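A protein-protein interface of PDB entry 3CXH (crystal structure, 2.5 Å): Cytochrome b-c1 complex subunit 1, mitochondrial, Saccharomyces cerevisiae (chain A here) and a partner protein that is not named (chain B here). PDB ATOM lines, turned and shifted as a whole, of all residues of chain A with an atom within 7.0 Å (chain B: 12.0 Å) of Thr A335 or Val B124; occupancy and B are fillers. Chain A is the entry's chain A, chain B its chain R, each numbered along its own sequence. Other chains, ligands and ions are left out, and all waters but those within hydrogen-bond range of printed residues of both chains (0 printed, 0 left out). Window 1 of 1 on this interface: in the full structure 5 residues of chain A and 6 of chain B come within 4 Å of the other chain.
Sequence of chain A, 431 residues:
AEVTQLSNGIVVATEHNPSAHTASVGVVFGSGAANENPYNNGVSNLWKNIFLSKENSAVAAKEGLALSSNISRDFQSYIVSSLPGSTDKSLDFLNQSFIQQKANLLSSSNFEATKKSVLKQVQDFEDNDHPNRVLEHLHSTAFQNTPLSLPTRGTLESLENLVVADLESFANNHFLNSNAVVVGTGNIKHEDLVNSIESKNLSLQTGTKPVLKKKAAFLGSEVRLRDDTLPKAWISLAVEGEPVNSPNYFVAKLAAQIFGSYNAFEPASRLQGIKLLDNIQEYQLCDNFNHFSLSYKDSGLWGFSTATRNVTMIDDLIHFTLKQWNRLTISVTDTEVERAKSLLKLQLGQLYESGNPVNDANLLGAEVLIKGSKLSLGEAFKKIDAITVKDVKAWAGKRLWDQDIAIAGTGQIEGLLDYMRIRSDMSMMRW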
ATOM      1  N   GLY A 273      10.876   7.052 -34.369  1.00  0.00           N
ATOM      2  CA  GLY A 273      10.709   6.432 -33.069  1.00  0.00           C
ATOM      3  C   GLY A 273       9.578   5.427 -33.063  1.00  0.00           C
ATOM      4  O   GLY A 273       8.583   5.597 -32.337  1.00  0.00           O
ATOM      5  N   LYS A 275       8.936   1.381 -32.548  1.00  0.00           N
ATOM      6  CA  LYS A 275       9.497   0.120 -32.047  1.00  0.00           C
ATOM      7  C   LYS A 275       9.645  -0.940 -33.146  1.00  0.00           C
ATOM      8  O   LYS A 275      10.691  -1.588 -33.270  1.00  0.00           O
ATOM      9  CB  LYS A 275       8.597  -0.437 -30.947  1.00  0.00           C
ATOM     10  CG  LYS A 275       9.201  -0.500 -29.571  1.00  0.00           C
ATOM     11  CD  LYS A 275       9.129   0.835 -28.861  1.00  0.00           C
ATOM     12  CE  LYS A 275       9.366   0.662 -27.370  1.00  0.00           C
ATOM     13  NZ  LYS A 275       9.658   1.966 -26.717  1.00  0.00           N
ATOM     14  N   VAL A 332       1.292  -0.462 -24.494  1.00  0.00           N
ATOM     15  CA  VAL A 332       1.676   0.761 -25.190  1.00  0.00           C
ATOM     16  C   VAL A 332       2.180   1.775 -24.148  1.00  0.00           C
ATOM     17  O   VAL A 332       1.576   1.936 -23.083  1.00  0.00           O
ATOM     18  CB  VAL A 332       0.506   1.327 -26.032  1.00  0.00           C
ATOM     19  CG1 VAL A 332      -0.654   1.732 -25.157  1.00  0.00           C
ATOM     20  CG2 VAL A 332       0.987   2.478 -26.892  1.00  0.00           C
ATOM     21  N   THR A 333       3.339   2.375 -24.408  1.00  0.00           N
ATOM     22  CA  THR A 333       3.912   3.331 -23.466  1.00  0.00           C
ATOM     23  C   THR A 333       3.381   4.736 -23.625  1.00  0.00           C
ATOM     24  O   THR A 333       2.975   5.159 -24.710  1.00  0.00           O
ATOM     25  CB  THR A 333       5.457   3.425 -23.544  1.00  0.00           C
ATOM     26  OG1 THR A 333       5.851   3.998 -24.799  1.00  0.00           O
ATOM     27  CG2 THR A 333       6.097   2.071 -23.362  1.00  0.00           C
ATOM     28  N   ASP A 334       3.487   5.474 -22.529  1.00  0.00           N
ATOM     29  CA  ASP A 334       3.055   6.851 -22.439  1.00  0.00           C
ATOM     30  C   ASP A 334       3.703   7.713 -23.518  1.00  0.00           C
ATOM     31  O   ASP A 334       3.020   8.483 -24.199  1.00  0.00           O
ATOM     32  CB  ASP A 334       3.428   7.380 -21.061  1.00  0.00           C
ATOM     33  CG  ASP A 334       2.649   8.598 -20.685  1.00  0.00           C
ATOM     34  OD1 ASP A 334       3.070   9.712 -21.073  1.00  0.00           O
ATOM     35  OD2 ASP A 334       1.616   8.433 -20.000  1.00  0.00           O
ATOM     36  N   THR A 335       5.010   7.553 -23.703  1.00  0.00           N
ATOM     37  CA  THR A 335       5.726   8.340 -24.698  1.00  0.00           C
ATOM     38  C   THR A 335       5.413   7.962 -26.156  1.00  0.00           C
ATOM     39  O   THR A 335       5.661   8.751 -27.075  1.00  0.00           O
ATOM     40  CB  THR A 335       7.260   8.421 -24.388  1.00  0.00           C
ATOM     41  OG1 THR A 335       8.019   7.850 -25.457  1.00  0.00           O
ATOM     42  CG2 THR A 335       7.589   7.722 -23.097  1.00  0.00           C
ATOM     43  N   GLU A 336       4.875   6.763 -26.369  1.00  0.00           N
ATOM     44  CA  GLU A 336       4.480   6.334 -27.711  1.00  0.00           C
ATOM     45  C   GLU A 336       3.186   7.087 -28.041  1.00  0.00           C
ATOM     46  O   GLU A 336       2.986   7.573 -29.163  1.00  0.00           O
ATOM     47  CB  GLU A 336       4.235   4.821 -27.759  1.00  0.00           C
ATOM     48  CG  GLU A 336       5.487   3.995 -28.080  1.00  0.00           C
ATOM     49  CD  GLU A 336       5.282   2.497 -27.902  1.00  0.00           C
ATOM     50  OE1 GLU A 336       4.833   2.068 -26.817  1.00  0.00           O
ATOM     51  OE2 GLU A 336       5.577   1.744 -28.849  1.00  0.00           O
ATOM     52  N   VAL A 337       2.326   7.191 -27.031  1.00  0.00           N
ATOM     53  CA  VAL A 337       1.057   7.893 -27.152  1.00  0.00           C
ATOM     54  C   VAL A 337       1.296   9.387 -27.370  1.00  0.00           C
ATOM     55  O   VAL A 337       0.636  10.005 -28.204  1.00  0.00           O
ATOM     56  CB  VAL A 337       0.165   7.653 -25.908  1.00  0.00           C
ATOM     57  CG1 VAL A 337      -0.965   8.657 -25.862  1.00  0.00           C
ATOM     58  CG2 VAL A 337      -0.414   6.238 -25.947  1.00  0.00           C
ATOM     59  N   GLU A 338       2.269   9.958 -26.663  1.00  0.00           N
ATOM     60  CA  GLU A 338       2.573  11.378 -26.822  1.00  0.00           C
ATOM     61  C   GLU A 338       3.175  11.702 -28.186  1.00  0.00           C
ATOM     62  O   GLU A 338       2.858  12.736 -28.775  1.00  0.00           O
ATOM     63  CB  GLU A 338       3.488  11.868 -25.705  1.00  0.00           C
ATOM     64  CG  GLU A 338       2.823  11.861 -24.334  1.00  0.00           C
ATOM     65  CD  GLU A 338       1.605  12.790 -24.241  1.00  0.00           C
ATOM     66  OE1 GLU A 338       0.537  12.319 -23.780  1.00  0.00           O
ATOM     67  OE2 GLU A 338       1.719  13.987 -24.610  1.00  0.00           O
ATOM     68  N   ARG A 339       4.012  10.806 -28.704  1.00  0.00           N
ATOM     69  CA  ARG A 339       4.640  11.014 -30.008  1.00  0.00           C
ATOM     70  C   ARG A 339       3.563  10.979 -31.084  1.00  0.00           C
ATOM     71  O   ARG A 339       3.630  11.715 -32.058  1.00  0.00           O
ATOM     72  CB  ARG A 339       5.677   9.920 -30.297  1.00  0.00           C
ATOM     73  CG  ARG A 339       6.587  10.236 -31.475  1.00  0.00           C
ATOM     74  CD  ARG A 339       7.195   8.991 -32.115  1.00  0.00           C
ATOM     75  NE  ARG A 339       6.200   8.270 -32.905  1.00  0.00           N
ATOM     76  CZ  ARG A 339       6.302   8.024 -34.208  1.00  0.00           C
ATOM     77  NH1 ARG A 339       5.327   7.373 -34.828  1.00  0.00           N
ATOM     78  NH2 ARG A 339       7.371   8.424 -34.889  1.00  0.00           N
ATOM     79  N   ALA A 340       2.569  10.118 -30.892  1.00  0.00           N
ATOM     80  CA  ALA A 340       1.470   9.971 -31.836  1.00  0.00           C
ATOM     81  C   ALA A 340       0.573  11.203 -31.834  1.00  0.00           C
ATOM     82  O   ALA A 340       0.086  11.620 -32.894  1.00  0.00           O
ATOM     83  CB  ALA A 340       0.665   8.735 -31.511  1.00  0.00           C
ATOM     84  N   VAL A 389      -3.301   6.577 -22.210  1.00  0.00           N
ATOM     85  CA  VAL A 389      -2.866   5.214 -22.470  1.00  0.00           C
ATOM     86  C   VAL A 389      -4.036   4.255 -22.245  1.00  0.00           C
ATOM     87  O   VAL A 389      -4.253   3.334 -23.042  1.00  0.00           O
ATOM     88  CB  VAL A 389      -1.681   4.841 -21.571  1.00  0.00           C
ATOM     89  CG1 VAL A 389      -1.280   3.401 -21.783  1.00  0.00           C
ATOM     90  CG2 VAL A 389      -0.511   5.750 -21.869  1.00  0.00           C
ATOM     91  N   GLU B 115      22.908   6.913 -27.162  1.00  0.00           N
ATOM     92  CA  GLU B 115      21.881   7.907 -27.432  1.00  0.00           C
ATOM     93  C   GLU B 115      20.611   7.213 -27.925  1.00  0.00           C
ATOM     94  O   GLU B 115      19.508   7.505 -27.452  1.00  0.00           O
ATOM     95  CB  GLU B 115      22.370   8.926 -28.462  1.00  0.00           C
ATOM     96  CG  GLU B 115      21.303   9.920 -28.903  1.00  0.00           C
ATOM     97  CD  GLU B 115      21.847  10.943 -29.879  1.00  0.00           C
ATOM     98  OE1 GLU B 115      22.321  10.540 -30.965  1.00  0.00           O
ATOM     99  OE2 GLU B 115      21.823  12.153 -29.548  1.00  0.00           O
ATOM    100  N   LYS B 116      20.780   6.272 -28.850  1.00  0.00           N
ATOM    101  CA  LYS B 116      19.647   5.540 -29.379  1.00  0.00           C
ATOM    102  C   LYS B 116      18.897   4.805 -28.271  1.00  0.00           C
ATOM    103  O   LYS B 116      17.681   4.717 -28.300  1.00  0.00           O
ATOM    104  CB  LYS B 116      20.090   4.564 -30.471  1.00  0.00           C
ATOM    105  CG  LYS B 116      18.994   3.585 -30.889  1.00  0.00           C
ATOM    106  CD  LYS B 116      19.207   3.038 -32.284  1.00  0.00           C
ATOM    107  CE  LYS B 116      18.187   1.928 -32.591  1.00  0.00           C
ATOM    108  NZ  LYS B 116      16.776   2.263 -32.218  1.00  0.00           N
ATOM    109  N   ASP B 117      19.624   4.322 -27.274  1.00  0.00           N
ATOM    110  CA  ASP B 117      19.009   3.601 -26.168  1.00  0.00           C
ATOM    111  C   ASP B 117      18.228   4.558 -25.265  1.00  0.00           C
ATOM    112  O   ASP B 117      17.152   4.225 -24.763  1.00  0.00           O
ATOM    113  CB  ASP B 117      20.084   2.856 -25.365  1.00  0.00           C
ATOM    114  CG  ASP B 117      19.496   1.986 -24.266  1.00  0.00           C
ATOM    115  OD1 ASP B 117      18.901   0.940 -24.607  1.00  0.00           O
ATOM    116  OD2 ASP B 117      19.620   2.348 -23.069  1.00  0.00           O
ATOM    117  N   GLU B 118      18.790   5.743 -25.055  1.00  0.00           N
ATOM    118  CA  GLU B 118      18.164   6.763 -24.228  1.00  0.00           C
ATOM    119  C   GLU B 118      16.902   7.281 -24.900  1.00  0.00           C
ATOM    120  O   GLU B 118      15.851   7.374 -24.270  1.00  0.00           O
ATOM    121  CB  GLU B 118      19.147   7.905 -23.968  1.00  0.00           C
ATOM    122  CG  GLU B 118      20.278   7.508 -23.028  1.00  0.00           C
ATOM    123  CD  GLU B 118      21.389   8.537 -22.947  1.00  0.00           C
ATOM    124  OE1 GLU B 118      21.745   9.143 -23.990  1.00  0.00           O
ATOM    125  OE2 GLU B 118      21.919   8.725 -21.831  1.00  0.00           O
ATOM    126  N   LEU B 119      17.008   7.586 -26.189  1.00  0.00           N
ATOM    127  CA  LEU B 119      15.874   8.066 -26.960  1.00  0.00           C
ATOM    128  C   LEU B 119      14.751   7.013 -27.045  1.00  0.00           C
ATOM    129  O   LEU B 119      13.568   7.365 -27.079  1.00  0.00           O
ATOM    130  CB  LEU B 119      16.334   8.489 -28.358  1.00  0.00           C
ATOM    131  CG  LEU B 119      17.327   9.660 -28.434  1.00  0.00           C
ATOM    132  CD1 LEU B 119      17.713   9.901 -29.871  1.00  0.00           C
ATOM    133  CD2 LEU B 119      16.731  10.931 -27.833  1.00  0.00           C
ATOM    134  N   ASP B 120      15.119   5.730 -27.069  1.00  0.00           N
ATOM    135  CA  ASP B 120      14.134   4.639 -27.126  1.00  0.00           C
ATOM    136  C   ASP B 120      13.376   4.527 -25.801  1.00  0.00           C
ATOM    137  O   ASP B 120      12.285   3.966 -25.750  1.00  0.00           O
ATOM    138  CB  ASP B 120      14.813   3.281 -27.379  1.00  0.00           C
ATOM    139  CG  ASP B 120      15.137   3.020 -28.848  1.00  0.00           C
ATOM    140  OD1 ASP B 120      14.714   3.795 -29.722  1.00  0.00           O
ATOM    141  OD2 ASP B 120      15.826   2.016 -29.136  1.00  0.00           O
ATOM    142  N   ASN B 121      13.970   5.042 -24.729  1.00  0.00           N
ATOM    143  CA  ASN B 121      13.364   4.949 -23.408  1.00  0.00           C
ATOM    144  C   ASN B 121      13.106   6.281 -22.713  1.00  0.00           C
ATOM    145  O   ASN B 121      12.987   6.320 -21.490  1.00  0.00           O
ATOM    146  CB  ASN B 121      14.227   4.056 -22.497  1.00  0.00           C
ATOM    147  CG  ASN B 121      14.435   2.648 -23.066  1.00  0.00           C
ATOM    148  OD1 ASN B 121      13.526   1.810 -23.043  1.00  0.00           O
ATOM    149  ND2 ASN B 121      15.640   2.383 -23.573  1.00  0.00           N
ATOM    150  N   ILE B 122      13.028   7.372 -23.470  1.00  0.00           N
ATOM    151  CA  ILE B 122      12.765   8.672 -22.858  1.00  0.00           C
ATOM    152  C   ILE B 122      11.373   8.712 -22.257  1.00  0.00           C
ATOM    153  O   ILE B 122      10.450   8.092 -22.773  1.00  0.00           O
ATOM    154  CB  ILE B 122      12.827   9.842 -23.865  1.00  0.00           C
ATOM    155  CG1 ILE B 122      11.999   9.514 -25.103  1.00  0.00           C
ATOM    156  CG2 ILE B 122      14.257  10.220 -24.179  1.00  0.00           C
ATOM    157  CD1 ILE B 122      11.774  10.695 -26.000  1.00  0.00           C
ATOM    158  N   GLU B 123      11.241   9.418 -21.142  1.00  0.00           N
ATOM    159  CA  GLU B 123       9.946   9.590 -20.497  1.00  0.00           C
ATOM    160  C   GLU B 123       9.491  10.985 -20.914  1.00  0.00           C
ATOM    161  O   GLU B 123      10.311  11.801 -21.329  1.00  0.00           O
ATOM    162  CB  GLU B 123      10.073   9.525 -18.969  1.00  0.00           C
ATOM    163  CG  GLU B 123      10.499   8.169 -18.399  1.00  0.00           C
ATOM    164  CD  GLU B 123      10.415   8.110 -16.866  1.00  0.00           C
ATOM    165  OE1 GLU B 123       9.860   7.116 -16.340  1.00  0.00           O
ATOM    166  OE2 GLU B 123      10.899   9.048 -16.184  1.00  0.00           O
ATOM    167  N   VAL B 124       8.191  11.244 -20.851  1.00  0.00           N
ATOM    168  CA  VAL B 124       7.660  12.561 -21.208  1.00  0.00           C
ATOM    169  C   VAL B 124       6.997  13.234 -20.012  1.00  0.00           C
ATOM    170  O   VAL B 124       6.279  12.587 -19.242  1.00  0.00           O
ATOM    171  CB  VAL B 124       6.640  12.484 -22.362  1.00  0.00           C
ATOM    172  CG1 VAL B 124       7.357  12.462 -23.694  1.00  0.00           C
ATOM    173  CG2 VAL B 124       5.769  11.243 -22.210  1.00  0.00           C
ATOM    174  N   SER B 125       7.258  14.529 -19.850  1.00  0.00           N
ATOM    175  CA  SER B 125       6.684  15.288 -18.743  1.00  0.00           C
ATOM    176  C   SER B 125       5.702  16.352 -19.225  1.00  0.00           C
ATOM    177  O   SER B 125       6.098  17.451 -19.626  1.00  0.00           O
ATOM    178  CB  SER B 125       7.782  15.931 -17.897  1.00  0.00           C
ATOM    179  OG  SER B 125       7.227  16.592 -16.770  1.00  0.00           O
ATOM    180  N   LYS B 126       4.417  16.007 -19.180  1.00  0.00           N
ATOM    181  CA  LYS B 126       3.336  16.899 -19.599  1.00  0.00           C
ATOM    182  C   LYS B 126       2.998  17.912 -18.496  1.00  0.00           C
ATOM    183  O   LYS B 126       2.382  18.950 -18.820  1.00  0.00           O
ATOM    184  CB  LYS B 126       2.079  16.090 -19.968  1.00  0.00           C
ATOM    185  CG  LYS B 126       2.193  15.179 -21.213  1.00  0.00           C
ATOM    186  CD  LYS B 126       3.164  13.996 -21.031  1.00  0.00           C
ATOM    187  CE  LYS B 126       2.747  13.030 -19.913  1.00  0.00           C
ATOM    188  NZ  LYS B 126       1.496  12.275 -20.214  1.00  0.00           N
ATOM    189  OXT LYS B 126       3.353  17.660 -17.322  1.00  0.00           O
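OE1 of Glu A338 lies within salt-bridge range of NZ of Lys B126. The backbone carbonyl oxygen (O) of Asp B120 sits at hydrogen-bond distance from the side-chain amino group (NZ) of Lys A275. OD1 of Asp A334 is in salt-bridge range of NZ of Lys B126 (3.1 Å).
NZ of Lys B116 lies within salt-bridge range of OD2 of Asp B120, at 3.2 Å.
Asp A334 touches Val B124. Ile B122 touches Thr A335 (O to CG2, 2.9 Å). Glu B123 touches Thr A335 (CA to CG2, 3.98 Å). Thr A335 touches Val B124. CG of Glu A338 touches CG2 of Val B124, 3.7 Å away.
Thr A335 touches three residues of chain B. Val B124 touches just these residues of chain A: Asp A334, Thr A335 and Glu A338. No residue of chain B comes within 4 Å of Val A337. Of the printed residues of chain A, Lys B126 touches Asp A334 (3.1 Å) and Glu A338 (3.6 Å). Of the printed residues of chain A, Ile B122 touches Thr A335. Printed residues of chain B within 4 Å of Lys A275: Asp B120 (3.4 Å). Gly A273 touches none of the printed residues of chain B. The nearest printed residue of chain A that does not touch Asp B120 is Thr A335 (5.8 Å).
Hydrophobic or aromatic side chains of chain B that line the printed part of chain A: Val B124.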
